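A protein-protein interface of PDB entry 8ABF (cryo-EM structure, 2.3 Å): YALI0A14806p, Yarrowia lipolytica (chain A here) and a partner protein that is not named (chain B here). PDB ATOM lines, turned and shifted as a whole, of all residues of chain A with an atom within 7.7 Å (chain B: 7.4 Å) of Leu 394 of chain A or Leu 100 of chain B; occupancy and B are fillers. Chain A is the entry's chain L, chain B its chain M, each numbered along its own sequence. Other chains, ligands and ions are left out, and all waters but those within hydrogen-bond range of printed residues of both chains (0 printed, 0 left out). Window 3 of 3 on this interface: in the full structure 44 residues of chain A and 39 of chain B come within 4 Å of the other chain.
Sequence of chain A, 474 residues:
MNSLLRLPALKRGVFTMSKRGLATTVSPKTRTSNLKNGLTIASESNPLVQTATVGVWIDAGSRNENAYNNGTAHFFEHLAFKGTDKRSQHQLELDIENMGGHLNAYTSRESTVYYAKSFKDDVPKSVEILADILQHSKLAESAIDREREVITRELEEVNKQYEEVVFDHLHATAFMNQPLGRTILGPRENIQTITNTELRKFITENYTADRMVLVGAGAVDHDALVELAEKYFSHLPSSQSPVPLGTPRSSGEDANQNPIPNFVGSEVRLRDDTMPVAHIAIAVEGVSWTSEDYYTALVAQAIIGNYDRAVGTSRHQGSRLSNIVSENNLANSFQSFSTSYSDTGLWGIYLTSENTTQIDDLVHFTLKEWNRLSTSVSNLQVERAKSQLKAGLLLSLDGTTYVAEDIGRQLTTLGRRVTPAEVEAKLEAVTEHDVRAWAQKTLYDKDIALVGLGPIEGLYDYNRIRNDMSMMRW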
ATOM      1  N   SER A  27      -5.768  16.839  -6.373  1.00  0.00           N
ATOM      2  CA  SER A  27      -4.951  17.885  -6.959  1.00  0.00           C
ATOM      3  C   SER A  27      -4.418  18.838  -5.883  1.00  0.00           C
ATOM      4  O   SER A  27      -5.072  19.031  -4.857  1.00  0.00           O
ATOM      5  CB  SER A  27      -5.773  18.616  -7.978  1.00  0.00           C
ATOM      6  OG  SER A  27      -4.958  19.472  -8.754  1.00  0.00           O
ATOM      7  N   SER A 387     -23.052  10.601 -12.375  1.00  0.00           N
ATOM      8  CA  SER A 387     -21.852   9.776 -12.463  1.00  0.00           C
ATOM      9  C   SER A 387     -20.918  10.283 -13.555  1.00  0.00           C
ATOM     10  O   SER A 387     -19.727  10.478 -13.327  1.00  0.00           O
ATOM     11  CB  SER A 387     -22.203   8.337 -12.708  1.00  0.00           C
ATOM     12  OG  SER A 387     -22.821   7.787 -11.563  1.00  0.00           O
ATOM     13  N   GLN A 388     -21.485  10.520 -14.729  1.00  0.00           N
ATOM     14  CA  GLN A 388     -20.753  11.011 -15.874  1.00  0.00           C
ATOM     15  C   GLN A 388     -20.149  12.399 -15.644  1.00  0.00           C
ATOM     16  O   GLN A 388     -19.172  12.705 -16.323  1.00  0.00           O
ATOM     17  CB  GLN A 388     -21.728  11.037 -17.040  1.00  0.00           C
ATOM     18  CG  GLN A 388     -21.065  11.361 -18.361  1.00  0.00           C
ATOM     19  CD  GLN A 388     -21.899  10.887 -19.524  1.00  0.00           C
ATOM     20  OE1 GLN A 388     -23.120  11.035 -19.542  1.00  0.00           O
ATOM     21  NE2 GLN A 388     -21.237  10.321 -20.523  1.00  0.00           N
ATOM     22  N   LEU A 389     -20.770  13.241 -14.794  1.00  0.00           N
ATOM     23  CA  LEU A 389     -20.377  14.641 -14.622  1.00  0.00           C
ATOM     24  C   LEU A 389     -19.303  14.770 -13.546  1.00  0.00           C
ATOM     25  O   LEU A 389     -18.414  15.617 -13.625  1.00  0.00           O
ATOM     26  CB  LEU A 389     -21.586  15.477 -14.193  1.00  0.00           C
ATOM     27  CG  LEU A 389     -22.381  16.200 -15.272  1.00  0.00           C
ATOM     28  CD1 LEU A 389     -23.520  16.973 -14.621  1.00  0.00           C
ATOM     29  CD2 LEU A 389     -21.492  17.146 -16.064  1.00  0.00           C
ATOM     30  N   LYS A 390     -19.421  13.931 -12.518  1.00  0.00           N
ATOM     31  CA  LYS A 390     -18.460  13.900 -11.436  1.00  0.00           C
ATOM     32  C   LYS A 390     -17.051  13.709 -12.002  1.00  0.00           C
ATOM     33  O   LYS A 390     -16.117  14.345 -11.530  1.00  0.00           O
ATOM     34  CB  LYS A 390     -18.951  12.933 -10.352  1.00  0.00           C
ATOM     35  CG  LYS A 390     -17.896  12.011  -9.758  1.00  0.00           C
ATOM     36  CD  LYS A 390     -17.068  12.682  -8.681  1.00  0.00           C
ATOM     37  CE  LYS A 390     -15.909  11.845  -8.191  1.00  0.00           C
ATOM     38  NZ  LYS A 390     -15.344  12.390  -6.932  1.00  0.00           N
ATOM     39  N   ALA A 391     -16.918  12.878 -13.039  1.00  0.00           N
ATOM     40  CA  ALA A 391     -15.638  12.689 -13.701  1.00  0.00           C
ATOM     41  C   ALA A 391     -15.402  13.794 -14.721  1.00  0.00           C
ATOM     42  O   ALA A 391     -14.301  14.323 -14.812  1.00  0.00           O
ATOM     43  CB  ALA A 391     -15.567  11.326 -14.335  1.00  0.00           C
ATOM     44  N   GLY A 392     -16.436  14.121 -15.495  1.00  0.00           N
ATOM     45  CA  GLY A 392     -16.303  15.085 -16.575  1.00  0.00           C
ATOM     46  C   GLY A 392     -15.745  16.440 -16.134  1.00  0.00           C
ATOM     47  O   GLY A 392     -14.985  17.051 -16.872  1.00  0.00           O
ATOM     48  N   LEU A 393     -16.145  16.912 -14.944  1.00  0.00           N
ATOM     49  CA  LEU A 393     -15.710  18.211 -14.442  1.00  0.00           C
ATOM     50  C   LEU A 393     -14.239  18.187 -14.021  1.00  0.00           C
ATOM     51  O   LEU A 393     -13.634  19.242 -13.842  1.00  0.00           O
ATOM     52  CB  LEU A 393     -16.625  18.655 -13.291  1.00  0.00           C
ATOM     53  CG  LEU A 393     -18.076  18.956 -13.679  1.00  0.00           C
ATOM     54  CD1 LEU A 393     -18.970  19.037 -12.454  1.00  0.00           C
ATOM     55  CD2 LEU A 393     -18.191  20.226 -14.507  1.00  0.00           C
ATOM     56  N   LEU A 394     -13.686  16.990 -13.814  1.00  0.00           N
ATOM     57  CA  LEU A 394     -12.293  16.832 -13.422  1.00  0.00           C
ATOM     58  C   LEU A 394     -11.416  16.558 -14.641  1.00  0.00           C
ATOM     59  O   LEU A 394     -10.307  17.089 -14.708  1.00  0.00           O
ATOM     60  CB  LEU A 394     -12.189  15.714 -12.384  1.00  0.00           C
ATOM     61  CG  LEU A 394     -12.982  15.970 -11.106  1.00  0.00           C
ATOM     62  CD1 LEU A 394     -12.906  14.770 -10.185  1.00  0.00           C
ATOM     63  CD2 LEU A 394     -12.504  17.228 -10.393  1.00  0.00           C
ATOM     64  N   LEU A 395     -11.944  15.752 -15.588  1.00  0.00           N
ATOM     65  CA  LEU A 395     -11.252  15.266 -16.779  1.00  0.00           C
ATOM     66  C   LEU A 395     -10.871  16.417 -17.709  1.00  0.00           C
ATOM     67  O   LEU A 395      -9.875  16.328 -18.425  1.00  0.00           O
ATOM     68  CB  LEU A 395     -12.147  14.264 -17.529  1.00  0.00           C
ATOM     69  CG  LEU A 395     -11.766  12.786 -17.422  1.00  0.00           C
ATOM     70  CD1 LEU A 395     -12.070  12.211 -16.048  1.00  0.00           C
ATOM     71  CD2 LEU A 395     -12.486  11.977 -18.484  1.00  0.00           C
ATOM     72  N   SER A 396     -11.735  17.431 -17.781  1.00  0.00           N
ATOM     73  CA  SER A 396     -11.521  18.599 -18.619  1.00  0.00           C
ATOM     74  C   SER A 396     -10.179  19.271 -18.322  1.00  0.00           C
ATOM     75  O   SER A 396      -9.542  19.805 -19.227  1.00  0.00           O
ATOM     76  CB  SER A 396     -12.682  19.552 -18.505  1.00  0.00           C
ATOM     77  OG  SER A 396     -13.174  19.596 -17.177  1.00  0.00           O
ATOM     78  N   LEU A 397      -9.741  19.239 -17.058  1.00  0.00           N
ATOM     79  CA  LEU A 397      -8.531  19.934 -16.642  1.00  0.00           C
ATOM     80  C   LEU A 397      -7.318  19.043 -16.855  1.00  0.00           C
ATOM     81  O   LEU A 397      -6.852  18.373 -15.938  1.00  0.00           O
ATOM     82  CB  LEU A 397      -8.654  20.289 -15.162  1.00  0.00           C
ATOM     83  CG  LEU A 397     -10.054  20.637 -14.684  1.00  0.00           C
ATOM     84  CD1 LEU A 397     -10.069  20.721 -13.174  1.00  0.00           C
ATOM     85  CD2 LEU A 397     -10.536  21.965 -15.253  1.00  0.00           C
ATOM     86  N   ASP A 398      -6.801  19.062 -18.091  1.00  0.00           N
ATOM     87  CA  ASP A 398      -5.707  18.217 -18.530  1.00  0.00           C
ATOM     88  C   ASP A 398      -4.358  18.925 -18.369  1.00  0.00           C
ATOM     89  O   ASP A 398      -3.594  18.621 -17.452  1.00  0.00           O
ATOM     90  CB  ASP A 398      -5.916  17.850 -19.999  1.00  0.00           C
ATOM     91  CG  ASP A 398      -7.162  17.024 -20.268  1.00  0.00           C
ATOM     92  OD1 ASP A 398      -7.244  15.881 -19.766  1.00  0.00           O
ATOM     93  OD2 ASP A 398      -8.059  17.539 -20.958  1.00  0.00           O
ATOM     94  N   VAL A 403      -6.000  24.262 -16.845  1.00  0.00           N
ATOM     95  CA  VAL A 403      -6.048  24.542 -15.425  1.00  0.00           C
ATOM     96  C   VAL A 403      -6.082  26.050 -15.224  1.00  0.00           C
ATOM     97  O   VAL A 403      -6.850  26.528 -14.401  1.00  0.00           O
ATOM     98  CB  VAL A 403      -4.877  23.885 -14.678  1.00  0.00           C
ATOM     99  CG1 VAL A 403      -4.781  24.339 -13.229  1.00  0.00           C
ATOM    100  CG2 VAL A 403      -4.954  22.376 -14.783  1.00  0.00           C
ATOM    101  N   VAL A 418     -13.591  26.899  -6.736  1.00  0.00           N
ATOM    102  CA  VAL A 418     -14.369  25.941  -5.978  1.00  0.00           C
ATOM    103  C   VAL A 418     -13.632  24.611  -6.039  1.00  0.00           C
ATOM    104  O   VAL A 418     -13.315  24.130  -7.126  1.00  0.00           O
ATOM    105  CB  VAL A 418     -15.806  25.862  -6.518  1.00  0.00           C
ATOM    106  CG1 VAL A 418     -16.673  24.905  -5.719  1.00  0.00           C
ATOM    107  CG2 VAL A 418     -16.439  27.242  -6.553  1.00  0.00           C
ATOM    108  N   THR A 419     -13.353  24.055  -4.850  1.00  0.00           N
ATOM    109  CA  THR A 419     -12.605  22.819  -4.667  1.00  0.00           C
ATOM    110  C   THR A 419     -13.403  21.656  -5.249  1.00  0.00           C
ATOM    111  O   THR A 419     -14.630  21.707  -5.241  1.00  0.00           O
ATOM    112  CB  THR A 419     -12.315  22.557  -3.180  1.00  0.00           C
ATOM    113  OG1 THR A 419     -13.541  22.375  -2.472  1.00  0.00           O
ATOM    114  CG2 THR A 419     -11.544  23.676  -2.518  1.00  0.00           C
ATOM    115  N   PRO A 420     -12.772  20.575  -5.761  1.00  0.00           N
ATOM    116  CA  PRO A 420     -13.530  19.431  -6.276  1.00  0.00           C
ATOM    117  C   PRO A 420     -14.458  18.761  -5.266  1.00  0.00           C
ATOM    118  O   PRO A 420     -15.446  18.153  -5.657  1.00  0.00           O
ATOM    119  CB  PRO A 420     -12.431  18.454  -6.696  1.00  0.00           C
ATOM    120  CG  PRO A 420     -11.276  19.361  -7.006  1.00  0.00           C
ATOM    121  CD  PRO A 420     -11.321  20.394  -5.904  1.00  0.00           C
ATOM    122  N   ALA A 421     -14.144  18.879  -3.973  1.00  0.00           N
ATOM    123  CA  ALA A 421     -14.984  18.310  -2.936  1.00  0.00           C
ATOM    124  C   ALA A 421     -16.311  19.064  -2.838  1.00  0.00           C
ATOM    125  O   ALA A 421     -17.344  18.447  -2.602  1.00  0.00           O
ATOM    126  CB  ALA A 421     -14.237  18.319  -1.632  1.00  0.00           C
ATOM    127  N   VAL A 423     -17.611  20.785  -5.340  1.00  0.00           N
ATOM    128  CA  VAL A 423     -18.293  20.491  -6.586  1.00  0.00           C
ATOM    129  C   VAL A 423     -18.949  19.114  -6.527  1.00  0.00           C
ATOM    130  O   VAL A 423     -20.004  18.900  -7.111  1.00  0.00           O
ATOM    131  CB  VAL A 423     -17.317  20.596  -7.764  1.00  0.00           C
ATOM    132  CG1 VAL A 423     -17.922  20.040  -9.037  1.00  0.00           C
ATOM    133  CG2 VAL A 423     -16.882  22.030  -7.971  1.00  0.00           C
ATOM    134  N   GLU A 424     -18.290  18.171  -5.859  1.00  0.00           N
ATOM    135  CA  GLU A 424     -18.818  16.821  -5.780  1.00  0.00           C
ATOM    136  C   GLU A 424     -20.057  16.820  -4.886  1.00  0.00           C
ATOM    137  O   GLU A 424     -20.998  16.073  -5.128  1.00  0.00           O
ATOM    138  CB  GLU A 424     -17.721  15.890  -5.276  1.00  0.00           C
ATOM    139  CG  GLU A 424     -17.883  14.442  -5.702  1.00  0.00           C
ATOM    140  CD  GLU A 424     -18.510  13.488  -4.695  1.00  0.00           C
ATOM    141  OE1 GLU A 424     -18.546  12.272  -4.986  1.00  0.00           O
ATOM    142  OE2 GLU A 424     -18.967  13.957  -3.626  1.00  0.00           O
ATOM    143  N   SER B  32      -3.257  14.204  -8.968  1.00  0.00           N
ATOM    144  CA  SER B  32      -4.429  14.660  -9.689  1.00  0.00           C
ATOM    145  C   SER B  32      -5.456  13.549  -9.590  1.00  0.00           C
ATOM    146  O   SER B  32      -5.066  12.393  -9.421  1.00  0.00           O
ATOM    147  CB  SER B  32      -4.095  15.000 -11.130  1.00  0.00           C
ATOM    148  OG  SER B  32      -4.602  14.038 -12.024  1.00  0.00           O
ATOM    149  N   PRO B  33      -6.766  13.837  -9.729  1.00  0.00           N
ATOM    150  CA  PRO B  33      -7.768  12.779  -9.734  1.00  0.00           C
ATOM    151  C   PRO B  33      -7.899  12.014 -11.049  1.00  0.00           C
ATOM    152  O   PRO B  33      -8.567  10.983 -11.047  1.00  0.00           O
ATOM    153  CB  PRO B  33      -9.068  13.509  -9.382  1.00  0.00           C
ATOM    154  CG  PRO B  33      -8.853  14.895  -9.938  1.00  0.00           C
ATOM    155  CD  PRO B  33      -7.371  15.176  -9.807  1.00  0.00           C
ATOM    156  N   ILE B  34      -7.214  12.454 -12.123  1.00  0.00           N
ATOM    157  CA  ILE B  34      -7.399  11.831 -13.429  1.00  0.00           C
ATOM    158  C   ILE B  34      -6.145  11.088 -13.881  1.00  0.00           C
ATOM    159  O   ILE B  34      -5.054  11.639 -13.910  1.00  0.00           O
ATOM    160  CB  ILE B  34      -7.928  12.807 -14.504  1.00  0.00           C
ATOM    161  CG1 ILE B  34      -7.107  14.097 -14.585  1.00  0.00           C
ATOM    162  CG2 ILE B  34      -9.404  13.073 -14.258  1.00  0.00           C
ATOM    163  CD1 ILE B  34      -7.393  14.973 -15.794  1.00  0.00           C
ATOM    164  N   SER B  35      -6.340   9.835 -14.293  1.00  0.00           N
ATOM    165  CA  SER B  35      -5.277   8.988 -14.803  1.00  0.00           C
ATOM    166  C   SER B  35      -5.452   8.773 -16.300  1.00  0.00           C
ATOM    167  O   SER B  35      -6.577   8.770 -16.800  1.00  0.00           O
ATOM    168  CB  SER B  35      -5.325   7.691 -14.082  1.00  0.00           C
ATOM    169  OG  SER B  35      -4.972   7.872 -12.717  1.00  0.00           O
ATOM    170  N   LEU B  79     -20.679   5.321 -17.100  1.00  0.00           N
ATOM    171  CA  LEU B  79     -20.905   5.309 -15.661  1.00  0.00           C
ATOM    172  C   LEU B  79     -19.664   5.693 -14.869  1.00  0.00           C
ATOM    173  O   LEU B  79     -19.780   6.106 -13.715  1.00  0.00           O
ATOM    174  CB  LEU B  79     -21.317   3.906 -15.245  1.00  0.00           C
ATOM    175  CG  LEU B  79     -22.700   3.505 -15.722  1.00  0.00           C
ATOM    176  CD1 LEU B  79     -23.037   2.109 -15.243  1.00  0.00           C
ATOM    177  CD2 LEU B  79     -23.759   4.507 -15.289  1.00  0.00           C
ATOM    178  N   PHE B  80     -18.478   5.474 -15.446  1.00  0.00           N
ATOM    179  CA  PHE B  80     -17.226   5.867 -14.819  1.00  0.00           C
ATOM    180  C   PHE B  80     -16.847   7.272 -15.274  1.00  0.00           C
ATOM    181  O   PHE B  80     -15.859   7.843 -14.807  1.00  0.00           O
ATOM    182  CB  PHE B  80     -16.123   4.913 -15.271  1.00  0.00           C
ATOM    183  CG  PHE B  80     -15.989   3.634 -14.484  1.00  0.00           C
ATOM    184  CD1 PHE B  80     -15.900   3.656 -13.100  1.00  0.00           C
ATOM    185  CD2 PHE B  80     -15.925   2.407 -15.128  1.00  0.00           C
ATOM    186  CE1 PHE B  80     -15.736   2.490 -12.371  1.00  0.00           C
ATOM    187  CE2 PHE B  80     -15.808   1.234 -14.396  1.00  0.00           C
ATOM    188  CZ  PHE B  80     -15.700   1.274 -13.020  1.00  0.00           C
ATOM    189  N   GLY B  81     -17.586   7.782 -16.261  1.00  0.00           N
ATOM    190  CA  GLY B  81     -17.255   9.042 -16.901  1.00  0.00           C
ATOM    191  C   GLY B  81     -15.907   9.009 -17.619  1.00  0.00           C
ATOM    192  O   GLY B  81     -15.327  10.062 -17.863  1.00  0.00           O
ATOM    193  N   GLY B  82     -15.407   7.811 -17.952  1.00  0.00           N
ATOM    194  CA  GLY B  82     -14.145   7.706 -18.676  1.00  0.00           C
ATOM    195  C   GLY B  82     -14.268   8.153 -20.135  1.00  0.00           C
ATOM    196  O   GLY B  82     -15.374   8.284 -20.647  1.00  0.00           O
ATOM    197  N   GLN B  98      -8.907   7.745 -20.393  1.00  0.00           N
ATOM    198  CA  GLN B  98      -8.764   8.729 -19.345  1.00  0.00           C
ATOM    199  C   GLN B  98      -9.887   8.482 -18.345  1.00  0.00           C
ATOM    200  O   GLN B  98     -11.032   8.335 -18.747  1.00  0.00           O
ATOM    201  CB  GLN B  98      -8.819  10.078 -20.048  1.00  0.00           C
ATOM    202  CG  GLN B  98      -8.541  11.254 -19.144  1.00  0.00           C
ATOM    203  CD  GLN B  98      -8.349  12.512 -19.954  1.00  0.00           C
ATOM    204  OE1 GLN B  98      -9.281  13.019 -20.574  1.00  0.00           O
ATOM    205  NE2 GLN B  98      -7.129  13.024 -19.952  1.00  0.00           N
ATOM    206  N   PHE B  99      -9.568   8.405 -17.054  1.00  0.00           N
ATOM    207  CA  PHE B  99     -10.572   8.035 -16.067  1.00  0.00           C
ATOM    208  C   PHE B  99     -10.155   8.601 -14.715  1.00  0.00           C
ATOM    209  O   PHE B  99      -9.078   9.157 -14.579  1.00  0.00           O
ATOM    210  CB  PHE B  99     -10.750   6.509 -16.004  1.00  0.00           C
ATOM    211  CG  PHE B  99      -9.441   5.764 -15.968  1.00  0.00           C
ATOM    212  CD1 PHE B  99      -8.774   5.479 -17.153  1.00  0.00           C
ATOM    213  CD2 PHE B  99      -8.852   5.398 -14.760  1.00  0.00           C
ATOM    214  CE1 PHE B  99      -7.535   4.854 -17.138  1.00  0.00           C
ATOM    215  CE2 PHE B  99      -7.614   4.769 -14.748  1.00  0.00           C
ATOM    216  CZ  PHE B  99      -6.952   4.514 -15.932  1.00  0.00           C
ATOM    217  N   LEU B 100     -10.983   8.405 -13.690  1.00  0.00           N
ATOM    218  CA  LEU B 100     -10.595   8.732 -12.322  1.00  0.00           C
ATOM    219  C   LEU B 100      -9.629   7.679 -11.784  1.00  0.00           C
ATOM    220  O   LEU B 100      -9.791   6.509 -12.097  1.00  0.00           O
ATOM    221  CB  LEU B 100     -11.853   8.805 -11.462  1.00  0.00           C
ATOM    222  CG  LEU B 100     -12.841   9.886 -11.887  1.00  0.00           C
ATOM    223  CD1 LEU B 100     -14.103   9.855 -11.048  1.00  0.00           C
ATOM    224  CD2 LEU B 100     -12.210  11.271 -11.840  1.00  0.00           C
ATOM    225  N   LYS B 101      -8.652   8.103 -10.963  1.00  0.00           N
ATOM    226  CA  LYS B 101      -7.538   7.283 -10.496  1.00  0.00           C
ATOM    227  C   LYS B 101      -8.026   5.913 -10.019  1.00  0.00           C
ATOM    228  O   LYS B 101      -7.508   4.873 -10.429  1.00  0.00           O
ATOM    229  CB  LYS B 101      -6.792   7.954  -9.329  1.00  0.00           C
ATOM    230  CG  LYS B 101      -5.403   8.510  -9.588  1.00  0.00           C
ATOM    231  CD  LYS B 101      -4.361   7.932  -8.641  1.00  0.00           C
ATOM    232  CE  LYS B 101      -3.034   8.655  -8.655  1.00  0.00           C
ATOM    233  NZ  LYS B 101      -3.161   9.992  -8.029  1.00  0.00           N
ATOM    234  N   GLN B 102      -9.070   5.929  -9.190  1.00  0.00           N
ATOM    235  CA  GLN B 102      -9.533   4.741  -8.498  1.00  0.00           C
ATOM    236  C   GLN B 102     -10.091   3.689  -9.457  1.00  0.00           C
ATOM    237  O   GLN B 102     -10.127   2.528  -9.087  1.00  0.00           O
ATOM    238  CB  GLN B 102     -10.535   5.097  -7.400  1.00  0.00           C
ATOM    239  CG  GLN B 102     -11.924   5.458  -7.894  1.00  0.00           C
ATOM    240  CD  GLN B 102     -12.090   6.926  -8.208  1.00  0.00           C
ATOM    241  OE1 GLN B 102     -11.224   7.757  -7.936  1.00  0.00           O
ATOM    242  NE2 GLN B 102     -13.200   7.253  -8.840  1.00  0.00           N
ATOM    243  N   ASP B 103     -10.477   4.060 -10.677  1.00  0.00           N
ATOM    244  CA  ASP B 103     -11.083   3.101 -11.596  1.00  0.00           C
ATOM    245  C   ASP B 103     -10.053   2.299 -12.399  1.00  0.00           C
ATOM    246  O   ASP B 103     -10.423   1.619 -13.357  1.00  0.00           O
ATOM    247  CB  ASP B 103     -12.017   3.815 -12.575  1.00  0.00           C
ATOM    248  CG  ASP B 103     -12.965   4.843 -11.975  1.00  0.00           C
ATOM    249  OD1 ASP B 103     -13.530   4.583 -10.887  1.00  0.00           O
ATOM    250  OD2 ASP B 103     -13.142   5.926 -12.626  1.00  0.00           O
ATOM    251  N   LEU B 104      -8.774   2.351 -12.004  1.00  0.00           N
ATOM    252  CA  LEU B 104      -7.694   1.728 -12.765  1.00  0.00           C
ATOM    253  C   LEU B 104      -7.944   0.251 -13.098  1.00  0.00           C
ATOM    254  O   LEU B 104      -7.770  -0.141 -14.253  1.00  0.00           O
ATOM    255  CB  LEU B 104      -6.360   1.919 -12.038  1.00  0.00           C
ATOM    256  CG  LEU B 104      -5.156   1.251 -12.701  1.00  0.00           C
ATOM    257  CD1 LEU B 104      -4.832   1.906 -14.042  1.00  0.00           C
ATOM    258  CD2 LEU B 104      -3.951   1.295 -11.778  1.00  0.00           C
ATOM    259  N   PRO B 105      -8.353  -0.628 -12.149  1.00  0.00           N
ATOM    260  CA  PRO B 105      -8.540  -2.050 -12.455  1.00  0.00           C
ATOM    261  C   PRO B 105      -9.502  -2.359 -13.600  1.00  0.00           C
ATOM    262  O   PRO B 105      -9.339  -3.364 -14.290  1.00  0.00           O
ATOM    263  CB  PRO B 105      -9.148  -2.602 -11.161  1.00  0.00           C
ATOM    264  CG  PRO B 105      -8.578  -1.713 -10.101  1.00  0.00           C
ATOM    265  CD  PRO B 105      -8.616  -0.342 -10.728  1.00  0.00           C
ATOM    266  N   PHE B 107     -10.027  -0.455 -16.276  1.00  0.00           N
ATOM    267  CA  PHE B 107      -9.405  -0.079 -17.539  1.00  0.00           C
ATOM    268  C   PHE B 107      -8.321  -1.062 -17.955  1.00  0.00           C
ATOM    269  O   PHE B 107      -8.127  -1.299 -19.147  1.00  0.00           O
ATOM    270  CB  PHE B 107      -8.998   1.396 -17.517  1.00  0.00           C
ATOM    271  CG  PHE B 107     -10.251   2.223 -17.495  1.00  0.00           C
ATOM    272  CD1 PHE B 107     -10.952   2.447 -18.670  1.00  0.00           C
ATOM    273  CD2 PHE B 107     -10.822   2.611 -16.292  1.00  0.00           C
ATOM    274  CE1 PHE B 107     -12.155   3.136 -18.647  1.00  0.00           C
ATOM    275  CE2 PHE B 107     -12.042   3.274 -16.265  1.00  0.00           C
ATOM    276  CZ  PHE B 107     -12.703   3.542 -17.447  1.00  0.00           C
ATOM    277  N   ASN B 197      -0.112   9.376 -14.181  1.00  0.00           N
ATOM    278  CA  ASN B 197      -0.784   9.606 -12.896  1.00  0.00           C
ATOM    279  C   ASN B 197      -1.383   8.295 -12.387  1.00  0.00           C
ATOM    280  O   ASN B 197      -2.503   8.237 -11.878  1.00  0.00           O
ATOM    281  CB  ASN B 197      -1.666  10.869 -12.852  1.00  0.00           C
ATOM    282  CG  ASN B 197      -2.445  11.099 -11.564  1.00  0.00           C
ATOM    283  OD1 ASN B 197      -1.896  11.401 -10.509  1.00  0.00           O
ATOM    284  ND2 ASN B 197      -3.763  11.024 -11.643  1.00  0.00           N
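The side-chain carboxylate (OD1) of Asp 398 of chain A lies within hydrogen-bond range of the side-chain amide nitrogen (NE2) of Gln 98 of chain B (2.9 Å).
The side-chain amide nitrogen (ND2) of Asn 197 of chain B sits at hydrogen-bond distance from the backbone carbonyl oxygen (O) of Ile 34 of chain B, 2.7 Å away. The side-chain hydroxyl (OG) of Ser 32 of chain B lies within hydrogen-bond range of the backbone NH (N) of Ile 34 of chain B (3.1 Å). N of Leu 100 of chain B sits close to OD2 of Asp 103 of chain B (3.5 Å). OE1 of Glu 424 of chain A is in salt-bridge range of NZ of Lys 390 of chain A (3.7 Å).
Among the printed residues, pairs that only touch across the chains: Ser 387 of chain A with Leu 79 of chain B (3.4 Å), Lys 390 of chain A with Leu 100 of chain B (3.9 Å), Ala 391 of chain A with Phe 80 of chain B (3.5 Å), Ala 391 of chain A with Gly 81 of chain B (3.8 Å), Ala 391 of chain A with Leu 100 of chain B (3.9 Å), Leu 394 of chain A with Ile 34 of chain B (3.8 Å), Leu 394 of chain A with Leu 100 of chain B (3.9 Å), Leu 395 of chain A with Ile 34 of chain B (3.3 Å), Leu 395 of chain A with Gly 81 of chain B (3.5 Å), Leu 395 of chain A with Gln 98 of chain B (3.9 Å) and Leu 397 of chain A with Ile 34 of chain B (3.4 Å).
Leu 100 of chain B touches three residues of chain A. Of the printed residues of chain A, Gln 98 of chain B touches Leu 395 and Asp 398. Of the printed residues of chain B, Ala 391 of chain A touches Phe 80 (3.5 Å), Gly 81 (3.8 Å) and Leu 100 (3.9 Å). The nearest residue of chain B that does not touch Leu 394 of chain A is Pro 33 of chain B (4.1 Å). The nearest printed residue of chain B that does not touch Leu 397 of chain A is Ser 32 of chain B (6.3 Å).
Hydrophobic or aromatic side chains of chain B that line the printed part of chain A: Ile 34 and Leu 100. Hydrophobic or aromatic side chains of chain A that line the printed part of chain B: Ala 391, Leu 394 and Leu 395. Among the printed residues, no Asp or Glu carboxylate lies within 4 Å of a Lys or Arg side-chain nitrogen of the other chain.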
